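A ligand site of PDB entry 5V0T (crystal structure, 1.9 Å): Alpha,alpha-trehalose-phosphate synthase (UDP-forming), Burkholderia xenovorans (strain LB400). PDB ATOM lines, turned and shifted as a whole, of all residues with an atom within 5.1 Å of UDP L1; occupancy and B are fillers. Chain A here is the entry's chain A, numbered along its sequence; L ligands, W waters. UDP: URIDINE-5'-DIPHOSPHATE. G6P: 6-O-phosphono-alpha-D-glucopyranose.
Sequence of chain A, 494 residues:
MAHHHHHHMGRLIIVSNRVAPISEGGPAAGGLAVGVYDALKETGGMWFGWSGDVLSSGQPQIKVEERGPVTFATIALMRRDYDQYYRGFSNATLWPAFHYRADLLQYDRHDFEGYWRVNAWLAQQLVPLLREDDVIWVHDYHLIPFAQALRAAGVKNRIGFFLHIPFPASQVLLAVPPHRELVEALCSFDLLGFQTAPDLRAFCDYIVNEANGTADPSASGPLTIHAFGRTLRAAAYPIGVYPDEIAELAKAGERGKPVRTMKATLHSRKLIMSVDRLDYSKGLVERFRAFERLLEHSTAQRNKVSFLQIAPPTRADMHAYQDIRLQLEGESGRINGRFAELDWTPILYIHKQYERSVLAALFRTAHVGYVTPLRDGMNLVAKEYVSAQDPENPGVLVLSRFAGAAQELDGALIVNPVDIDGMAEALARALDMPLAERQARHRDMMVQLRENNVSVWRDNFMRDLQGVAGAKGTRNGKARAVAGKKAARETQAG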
ATOM      1  N   PRO A  27      -2.479 -27.089 -13.411  1.00  0.00           N
ATOM      2  CA  PRO A  27      -2.316 -26.311 -14.645  1.00  0.00           C
ATOM      3  C   PRO A  27      -0.996 -25.559 -14.702  1.00  0.00           C
ATOM      4  O   PRO A  27      -0.540 -25.068 -13.666  1.00  0.00           O
ATOM      5  CB  PRO A  27      -3.480 -25.330 -14.583  1.00  0.00           C
ATOM      6  CG  PRO A  27      -3.704 -25.120 -13.109  1.00  0.00           C
ATOM      7  CD  PRO A  27      -3.417 -26.465 -12.472  1.00  0.00           C
ATOM      8  N   ALA A  28      -0.407 -25.451 -15.892  1.00  0.00           N
ATOM      9  CA  ALA A  28       0.850 -24.740 -16.100  1.00  0.00           C
ATOM     10  C   ALA A  28       0.647 -23.615 -17.096  1.00  0.00           C
ATOM     11  O   ALA A  28      -0.038 -23.783 -18.108  1.00  0.00           O
ATOM     12  CB  ALA A  28       1.960 -25.679 -16.595  1.00  0.00           C
ATOM     13  N   ALA A  29       1.247 -22.457 -16.800  1.00  0.00           N
ATOM     14  CA  ALA A  29       1.184 -21.333 -17.723  1.00  0.00           C
ATOM     15  C   ALA A  29       2.360 -21.396 -18.687  1.00  0.00           C
ATOM     16  O   ALA A  29       3.507 -21.610 -18.269  1.00  0.00           O
ATOM     17  CB  ALA A  29       1.183 -20.011 -16.959  1.00  0.00           C
ATOM     18  N   GLY A  30       2.074 -21.226 -19.977  1.00  0.00           N
ATOM     19  CA  GLY A  30       3.113 -21.216 -20.986  1.00  0.00           C
ATOM     20  C   GLY A  30       2.537 -21.725 -22.291  1.00  0.00           C
ATOM     21  O   GLY A  30       1.914 -22.788 -22.309  1.00  0.00           O
ATOM     22  N   GLY A  31       2.729 -20.972 -23.382  1.00  0.00           N
ATOM     23  CA  GLY A  31       2.104 -21.316 -24.642  1.00  0.00           C
ATOM     24  C   GLY A  31       2.814 -22.402 -25.432  1.00  0.00           C
ATOM     25  O   GLY A  31       2.185 -23.087 -26.253  1.00  0.00           O
ATOM     26  N   LEU A  32       4.109 -22.578 -25.216  1.00  0.00           N
ATOM     27  CA  LEU A  32       4.797 -23.689 -25.874  1.00  0.00           C
ATOM     28  C   LEU A  32       4.144 -25.013 -25.512  1.00  0.00           C
ATOM     29  O   LEU A  32       3.767 -25.798 -26.392  1.00  0.00           O
ATOM     30  CB  LEU A  32       6.304 -23.704 -25.510  1.00  0.00           C
ATOM     31  CG  LEU A  32       7.141 -24.851 -26.122  1.00  0.00           C
ATOM     32  CD1 LEU A  32       8.589 -24.440 -26.322  1.00  0.00           C
ATOM     33  CD2 LEU A  32       7.066 -26.203 -25.320  1.00  0.00           C
ATOM     34  N   VAL A  34       1.237 -25.698 -24.316  1.00  0.00           N
ATOM     35  CA  VAL A  34      -0.133 -25.765 -24.808  1.00  0.00           C
ATOM     36  C   VAL A  34      -0.159 -26.063 -26.302  1.00  0.00           C
ATOM     37  O   VAL A  34      -0.854 -26.970 -26.767  1.00  0.00           O
ATOM     38  CB  VAL A  34      -0.893 -24.470 -24.479  1.00  0.00           C
ATOM     39  CG1 VAL A  34      -2.203 -24.405 -25.254  1.00  0.00           C
ATOM     40  CG2 VAL A  34      -1.169 -24.376 -22.974  1.00  0.00           C
ATOM     41  N   TRP A  95      16.434 -15.038 -22.975  1.00  0.00           N
ATOM     42  CA  TRP A  95      15.072 -14.499 -22.843  1.00  0.00           C
ATOM     43  C   TRP A  95      15.062 -12.970 -22.817  1.00  0.00           C
ATOM     44  O   TRP A  95      14.325 -12.380 -23.620  1.00  0.00           O
ATOM     45  CB  TRP A  95      14.373 -15.072 -21.605  1.00  0.00           C
ATOM     46  CG  TRP A  95      12.967 -14.517 -21.452  1.00  0.00           C
ATOM     47  CD1 TRP A  95      12.604 -13.404 -20.761  1.00  0.00           C
ATOM     48  CD2 TRP A  95      11.765 -15.055 -22.021  1.00  0.00           C
ATOM     49  NE1 TRP A  95      11.242 -13.206 -20.851  1.00  0.00           N
ATOM     50  CE2 TRP A  95      10.709 -14.211 -21.613  1.00  0.00           C
ATOM     51  CE3 TRP A  95      11.476 -16.175 -22.803  1.00  0.00           C
ATOM     52  CZ2 TRP A  95       9.370 -14.447 -21.978  1.00  0.00           C
ATOM     53  CZ3 TRP A  95      10.140 -16.428 -23.159  1.00  0.00           C
ATOM     54  CH2 TRP A  95       9.111 -15.553 -22.765  1.00  0.00           C
ATOM     55  N   VAL A 275      -4.569 -12.194 -18.858  1.00  0.00           N
ATOM     56  CA  VAL A 275      -3.959 -13.422 -18.360  1.00  0.00           C
ATOM     57  C   VAL A 275      -2.542 -13.466 -18.886  1.00  0.00           C
ATOM     58  O   VAL A 275      -2.347 -13.546 -20.101  1.00  0.00           O
ATOM     59  CB  VAL A 275      -4.703 -14.694 -18.820  1.00  0.00           C
ATOM     60  CG1 VAL A 275      -3.983 -15.913 -18.266  1.00  0.00           C
ATOM     61  CG2 VAL A 275      -6.169 -14.690 -18.380  1.00  0.00           C
ATOM     62  N   ARG A 277       1.640 -14.843 -17.635  1.00  0.00           N
ATOM     63  CA  ARG A 277       2.759 -15.082 -16.709  1.00  0.00           C
ATOM     64  C   ARG A 277       3.300 -13.714 -16.275  1.00  0.00           C
ATOM     65  O   ARG A 277       3.338 -12.771 -17.071  1.00  0.00           O
ATOM     66  CB  ARG A 277       3.858 -15.909 -17.378  1.00  0.00           C
ATOM     67  CG  ARG A 277       3.522 -17.387 -17.637  1.00  0.00           C
ATOM     68  CD  ARG A 277       4.745 -18.137 -18.253  1.00  0.00           C
ATOM     69  NE  ARG A 277       5.182 -17.436 -19.462  1.00  0.00           N
ATOM     70  CZ  ARG A 277       6.230 -16.625 -19.535  1.00  0.00           C
ATOM     71  NH1 ARG A 277       7.010 -16.429 -18.470  1.00  0.00           N
ATOM     72  NH2 ARG A 277       6.496 -16.010 -20.671  1.00  0.00           N
ATOM     73  N   LYS A 282       5.714  -8.863 -20.582  1.00  0.00           N
ATOM     74  CA  LYS A 282       4.277  -8.746 -20.809  1.00  0.00           C
ATOM     75  C   LYS A 282       3.735  -7.317 -20.648  1.00  0.00           C
ATOM     76  O   LYS A 282       2.534  -7.096 -20.821  1.00  0.00           O
ATOM     77  CB  LYS A 282       3.537  -9.701 -19.863  1.00  0.00           C
ATOM     78  CG  LYS A 282       3.942 -11.183 -20.094  1.00  0.00           C
ATOM     79  CD  LYS A 282       3.365 -11.734 -21.392  1.00  0.00           C
ATOM     80  CE  LYS A 282       3.770 -13.217 -21.623  1.00  0.00           C
ATOM     81  NZ  LYS A 282       3.297 -13.758 -22.951  1.00  0.00           N
ATOM     82  N   ILE A 310      -5.028 -11.858 -14.114  1.00  0.00           N
ATOM     83  CA  ILE A 310      -4.499 -13.127 -13.632  1.00  0.00           C
ATOM     84  C   ILE A 310      -3.042 -13.184 -14.063  1.00  0.00           C
ATOM     85  O   ILE A 310      -2.728 -13.092 -15.258  1.00  0.00           O
ATOM     86  CB  ILE A 310      -5.314 -14.300 -14.167  1.00  0.00           C
ATOM     87  CG1 ILE A 310      -6.736 -14.238 -13.605  1.00  0.00           C
ATOM     88  CG2 ILE A 310      -4.648 -15.637 -13.785  1.00  0.00           C
ATOM     89  CD1 ILE A 310      -7.675 -15.383 -14.077  1.00  0.00           C
ATOM     90  N   PRO A 312       0.074 -15.463 -13.131  1.00  0.00           N
ATOM     91  CA  PRO A 312       0.652 -16.557 -12.366  1.00  0.00           C
ATOM     92  C   PRO A 312       2.149 -16.390 -12.173  1.00  0.00           C
ATOM     93  O   PRO A 312       2.830 -15.768 -13.004  1.00  0.00           O
ATOM     94  CB  PRO A 312       0.349 -17.794 -13.242  1.00  0.00           C
ATOM     95  CG  PRO A 312      -0.235 -17.311 -14.486  1.00  0.00           C
ATOM     96  CD  PRO A 312      -0.714 -15.928 -14.276  1.00  0.00           C
ATOM     97  N   LYS A 352      -1.750 -16.290  -9.295  1.00  0.00           N
ATOM     98  CA  LYS A 352      -1.986 -17.742  -9.262  1.00  0.00           C
ATOM     99  C   LYS A 352      -2.317 -18.246 -10.664  1.00  0.00           C
ATOM    100  O   LYS A 352      -2.823 -17.511 -11.505  1.00  0.00           O
ATOM    101  CB  LYS A 352      -3.134 -18.117  -8.298  1.00  0.00           C
ATOM    102  CG  LYS A 352      -2.813 -17.882  -6.824  1.00  0.00           C
ATOM    103  CD  LYS A 352      -3.944 -18.347  -5.906  1.00  0.00           C
ATOM    104  CE  LYS A 352      -4.686 -17.168  -5.279  1.00  0.00           C
ATOM    105  NZ  LYS A 352      -5.708 -17.609  -4.277  1.00  0.00           N
ATOM    106  N   GLN A 353      -2.064 -19.534 -10.897  1.00  0.00           N
ATOM    107  CA  GLN A 353      -2.400 -20.171 -12.158  1.00  0.00           C
ATOM    108  C   GLN A 353      -3.820 -20.713 -12.109  1.00  0.00           C
ATOM    109  O   GLN A 353      -4.323 -21.102 -11.048  1.00  0.00           O
ATOM    110  CB  GLN A 353      -1.433 -21.316 -12.489  1.00  0.00           C
ATOM    111  N   TYR A 354      -4.471 -20.728 -13.272  1.00  0.00           N
ATOM    112  CA  TYR A 354      -5.813 -21.259 -13.419  1.00  0.00           C
ATOM    113  C   TYR A 354      -5.830 -22.322 -14.511  1.00  0.00           C
ATOM    114  O   TYR A 354      -5.008 -22.328 -15.430  1.00  0.00           O
ATOM    115  CB  TYR A 354      -6.821 -20.155 -13.773  1.00  0.00           C
ATOM    116  CG  TYR A 354      -7.209 -19.317 -12.599  1.00  0.00           C
ATOM    117  CD1 TYR A 354      -6.330 -18.372 -12.061  1.00  0.00           C
ATOM    118  CD2 TYR A 354      -8.464 -19.464 -11.999  1.00  0.00           C
ATOM    119  CE1 TYR A 354      -6.694 -17.600 -10.977  1.00  0.00           C
ATOM    120  CE2 TYR A 354      -8.836 -18.703 -10.913  1.00  0.00           C
ATOM    121  CZ  TYR A 354      -7.953 -17.767 -10.417  1.00  0.00           C
ATOM    122  OH  TYR A 354      -8.315 -17.004  -9.328  1.00  0.00           O
ATOM    123  N   GLU A 355      -6.815 -23.218 -14.420  1.00  0.00           N
ATOM    124  CA  GLU A 355      -7.046 -24.153 -15.498  1.00  0.00           C
ATOM    125  C   GLU A 355      -7.415 -23.407 -16.770  1.00  0.00           C
ATOM    126  O   GLU A 355      -8.139 -22.404 -16.752  1.00  0.00           O
ATOM    127  CB  GLU A 355      -8.160 -25.140 -15.113  1.00  0.00           C
ATOM    128  CG  GLU A 355      -7.751 -26.127 -14.032  1.00  0.00           C
ATOM    129  CD  GLU A 355      -6.800 -27.217 -14.539  1.00  0.00           C
ATOM    130  OE1 GLU A 355      -6.230 -27.953 -13.693  1.00  0.00           O
ATOM    131  OE2 GLU A 355      -6.636 -27.358 -15.775  1.00  0.00           O
ATOM    132  N   ARG A 356      -6.897 -23.911 -17.899  1.00  0.00           N
ATOM    133  CA  ARG A 356      -7.161 -23.266 -19.173  1.00  0.00           C
ATOM    134  C   ARG A 356      -8.652 -23.282 -19.492  1.00  0.00           C
ATOM    135  O   ARG A 356      -9.184 -22.342 -20.084  1.00  0.00           O
ATOM    136  CB  ARG A 356      -6.358 -23.982 -20.258  1.00  0.00           C
ATOM    137  CG  ARG A 356      -6.279 -23.253 -21.565  1.00  0.00           C
ATOM    138  CD  ARG A 356      -5.181 -23.830 -22.432  1.00  0.00           C
ATOM    139  NE  ARG A 356      -5.340 -23.405 -23.808  1.00  0.00           N
ATOM    140  CZ  ARG A 356      -5.789 -24.180 -24.782  1.00  0.00           C
ATOM    141  NH1 ARG A 356      -6.129 -25.435 -24.518  1.00  0.00           N
ATOM    142  NH2 ARG A 356      -5.899 -23.713 -26.002  1.00  0.00           N
ATOM    143  N   LEU A 359     -10.163 -20.368 -17.702  1.00  0.00           N
ATOM    144  CA  LEU A 359      -9.828 -19.107 -18.349  1.00  0.00           C
ATOM    145  C   LEU A 359     -10.684 -18.884 -19.592  1.00  0.00           C
ATOM    146  O   LEU A 359     -11.115 -17.758 -19.870  1.00  0.00           O
ATOM    147  CB  LEU A 359      -8.348 -19.069 -18.731  1.00  0.00           C
ATOM    148  CG  LEU A 359      -7.316 -19.066 -17.599  1.00  0.00           C
ATOM    149  CD1 LEU A 359      -5.916 -19.106 -18.180  1.00  0.00           C
ATOM    150  CD2 LEU A 359      -7.493 -17.857 -16.682  1.00  0.00           C
ATOM    151  N   ASP A 376       6.423 -10.249 -27.776  1.00  0.00           N
ATOM    152  CA  ASP A 376       5.833 -11.575 -27.587  1.00  0.00           C
ATOM    153  C   ASP A 376       5.924 -12.314 -28.912  1.00  0.00           C
ATOM    154  O   ASP A 376       5.542 -11.760 -29.959  1.00  0.00           O
ATOM    155  CB  ASP A 376       4.372 -11.458 -27.127  1.00  0.00           C
ATOM    156  CG  ASP A 376       3.891 -12.676 -26.361  1.00  0.00           C
ATOM    157  OD1 ASP A 376       4.190 -13.805 -26.825  1.00  0.00           O
ATOM    158  OD2 ASP A 376       3.212 -12.507 -25.314  1.00  0.00           O
ATOM    159  N   ASN A 379       1.676 -14.951 -28.641  1.00  0.00           N
ATOM    160  CA  ASN A 379       0.685 -14.710 -27.596  1.00  0.00           C
ATOM    161  C   ASN A 379      -0.580 -15.517 -27.880  1.00  0.00           C
ATOM    162  O   ASN A 379      -1.474 -15.094 -28.616  1.00  0.00           O
ATOM    163  CB  ASN A 379       0.352 -13.213 -27.400  1.00  0.00           C
ATOM    164  CG  ASN A 379      -0.368 -12.972 -26.072  1.00  0.00           C
ATOM    165  OD1 ASN A 379      -1.515 -13.376 -25.910  1.00  0.00           O
ATOM    166  ND2 ASN A 379       0.301 -12.324 -25.134  1.00  0.00           N
ATOM    167  N   LEU A 380      -0.643 -16.718 -27.296  1.00  0.00           N
ATOM    168  CA  LEU A 380      -1.817 -17.567 -27.485  1.00  0.00           C
ATOM    169  C   LEU A 380      -3.030 -17.016 -26.750  1.00  0.00           C
ATOM    170  O   LEU A 380      -4.167 -17.231 -27.191  1.00  0.00           O
ATOM    171  CB  LEU A 380      -1.517 -18.987 -26.998  1.00  0.00           C
ATOM    172  CG  LEU A 380      -0.513 -19.821 -27.812  1.00  0.00           C
ATOM    173  CD1 LEU A 380      -0.504 -21.236 -27.264  1.00  0.00           C
ATOM    174  CD2 LEU A 380      -0.858 -19.821 -29.286  1.00  0.00           C
ATOM    175  N   VAL A 381      -2.824 -16.285 -25.648  1.00  0.00           N
ATOM    176  CA  VAL A 381      -3.952 -15.747 -24.894  1.00  0.00           C
ATOM    177  C   VAL A 381      -4.805 -14.844 -25.785  1.00  0.00           C
ATOM    178  O   VAL A 381      -6.033 -14.865 -25.717  1.00  0.00           O
ATOM    179  CB  VAL A 381      -3.459 -15.012 -23.635  1.00  0.00           C
ATOM    180  CG1 VAL A 381      -4.498 -13.952 -23.165  1.00  0.00           C
ATOM    181  CG2 VAL A 381      -3.151 -16.035 -22.510  1.00  0.00           C
ATOM    182  N   GLU A 384      -6.847 -17.173 -27.906  1.00  0.00           N
ATOM    183  CA  GLU A 384      -7.833 -17.827 -27.039  1.00  0.00           C
ATOM    184  C   GLU A 384      -8.955 -16.866 -26.631  1.00  0.00           C
ATOM    185  O   GLU A 384     -10.122 -17.265 -26.586  1.00  0.00           O
ATOM    186  CB  GLU A 384      -7.137 -18.392 -25.804  1.00  0.00           C
ATOM    187  CG  GLU A 384      -6.175 -19.566 -26.125  1.00  0.00           C
ATOM    188  CD  GLU A 384      -5.275 -19.951 -24.943  1.00  0.00           C
ATOM    189  OE1 GLU A 384      -4.465 -20.888 -25.095  1.00  0.00           O
ATOM    190  OE2 GLU A 384      -5.366 -19.322 -23.875  1.00  0.00           O
HETATM  191  N1  UDP L   1      -2.365 -20.346 -19.230  1.00  0.00           N
HETATM  192  C2  UDP L   1      -2.918 -21.323 -18.417  1.00  0.00           C
HETATM  193  N3  UDP L   1      -3.116 -20.949 -17.113  1.00  0.00           N
HETATM  194  C4  UDP L   1      -2.821 -19.727 -16.553  1.00  0.00           C
HETATM  195  C5  UDP L   1      -2.246 -18.770 -17.454  1.00  0.00           C
HETATM  196  C6  UDP L   1      -2.059 -19.092 -18.739  1.00  0.00           C
HETATM  197  O2  UDP L   1      -3.209 -22.427 -18.816  1.00  0.00           O
HETATM  198  O4  UDP L   1      -3.051 -19.546 -15.353  1.00  0.00           O
HETATM  199  C1' UDP L   1      -2.147 -20.681 -20.637  1.00  0.00           C
HETATM  200  C2' UDP L   1      -2.927 -19.807 -21.602  1.00  0.00           C
HETATM  201  O2' UDP L   1      -4.245 -20.323 -21.770  1.00  0.00           O
HETATM  202  C3' UDP L   1      -2.076 -19.931 -22.867  1.00  0.00           C
HETATM  203  C4' UDP L   1      -0.651 -20.023 -22.302  1.00  0.00           C
HETATM  204  O4' UDP L   1      -0.785 -20.469 -20.937  1.00  0.00           O
HETATM  205  O3' UDP L   1      -2.358 -21.112 -23.617  1.00  0.00           O
HETATM  206  C5' UDP L   1       0.133 -18.741 -22.339  1.00  0.00           C
HETATM  207  O5' UDP L   1       0.695 -18.626 -23.662  1.00  0.00           O
HETATM  208  PA  UDP L   1       1.062 -17.207 -24.274  1.00  0.00           P
HETATM  209  O1A UDP L   1      -0.067 -16.222 -24.081  1.00  0.00           O
HETATM  210  O2A UDP L   1       1.472 -17.452 -25.687  1.00  0.00           O
HETATM  211  O3A UDP L   1       2.273 -16.667 -23.418  1.00  0.00           O
HETATM  212  PB  UDP L   1       3.559 -17.318 -22.762  1.00  0.00           P
HETATM  213  O1B UDP L   1       3.923 -18.463 -23.711  1.00  0.00           O
HETATM  214  O2B UDP L   1       4.604 -16.189 -22.876  1.00  0.00           O
HETATM  215  O3B UDP L   1       3.296 -17.757 -21.373  1.00  0.00           O
HETATM  216  C1  G6P L   2       7.292 -19.253 -23.118  1.00  0.00           C
HETATM  217  C2  G6P L   2       8.475 -19.967 -23.744  1.00  0.00           C
HETATM  218  C3  G6P L   2       8.406 -21.471 -23.460  1.00  0.00           C
HETATM  219  C4  G6P L   2       8.294 -21.693 -21.952  1.00  0.00           C
HETATM  220  C5  G6P L   2       7.097 -20.921 -21.406  1.00  0.00           C
HETATM  221  C6  G6P L   2       6.928 -21.163 -19.902  1.00  0.00           C
HETATM  222  O1  G6P L   2       6.120 -19.775 -23.729  1.00  0.00           O
HETATM  223  O2  G6P L   2       8.502 -19.705 -25.153  1.00  0.00           O
HETATM  224  O3  G6P L   2       9.613 -22.068 -23.952  1.00  0.00           O
HETATM  225  O4  G6P L   2       8.091 -23.096 -21.679  1.00  0.00           O
HETATM  226  O5  G6P L   2       7.244 -19.525 -21.701  1.00  0.00           O
HETATM  227  O6  G6P L   2       8.153 -20.833 -19.215  1.00  0.00           O
HETATM  228  P   G6P L   2       8.884 -21.955 -18.323  1.00  0.00           P
HETATM  229  O1P G6P L   2       8.033 -22.134 -17.096  1.00  0.00           O
HETATM  230  O2P G6P L   2      10.246 -21.378 -18.069  1.00  0.00           O
HETATM  231  O3P G6P L   2       8.903 -23.192 -19.189  1.00  0.00           O
HETATM  232  O   HOH W   1      -0.863 -16.483 -19.775  1.00  0.00           O
HETATM  233  O   HOH W   2       1.652 -15.786 -20.260  1.00  0.00           O
HETATM  234  O   HOH W   3       0.419 -14.373 -22.307  1.00  0.00           O
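Merely in contact with UDP L1: Gln 353 (3.3 Å), Asn 379 (3.4 Å), Val 275 (3.4 Å), Leu 359 (3.5 Å), Ala 28 (3.5 Å), Val 34 (3.5 Å), Arg 356 (3.6 Å), Ala 29 (3.7 Å) and Pro 312 (3.7 Å). The nearest printed residue that does not touch UDP L1 is Lys 352 (4.4 Å).
An oxygen (O2B) of UDP L1 is in salt-bridge range of the side-chain amino group (NZ) of Lys 282. The backbone NH of Gly 31 is in hydrogen-bond range of an oxygen (O1B) of UDP L1. NE of Arg 277 lies within salt-bridge range of O3B of UDP L1 (2.7 Å). The side-chain carboxylate (OE1) of Glu 384 lies within hydrogen-bond range of an oxygen (O3') of UDP L1. The backbone NH (N) of Gly 30 lies within hydrogen-bond range of an oxygen (O4') of UDP L1, at 3.1 Å. N of Val 381 sits at hydrogen-bond distance from O1A of UDP L1, 3.2 Å away. O4 of UDP L1 is in hydrogen-bond range of N of Tyr 354, 2.8 Å away. O of Tyr 354 sits at hydrogen-bond distance from N3 of UDP L1, at 2.9 Å. The backbone NH (N) of Leu 380 sits at hydrogen-bond distance from an oxygen (O2A) of UDP L1 (2.8 Å).
Water W3 lies within hydrogen-bond range of O1A of UDP L1, NZ of Lys 282 and ND2 of Asn 379. Water W2 bridges the backbone NH (N) of Arg 277 and an oxygen (O3B) of UDP L1.
O1B of UDP L1 is in hydrogen-bond range of O1 of G6P L2.
The side-chain amino group (NZ) of Lys 282 is in salt-bridge range of the side-chain carboxylate (OD2) of Asp 376, 2.7 Å away. OE1 of Glu 384 lies within salt-bridge range of NE of Arg 356, at 3.0 Å. ND2 of Asn 379 is in hydrogen-bond range of OD2 of Asp 376 (2.9 Å). N of Val 381 sits at hydrogen-bond distance from OD1 of Asn 379, 3.2 Å away.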
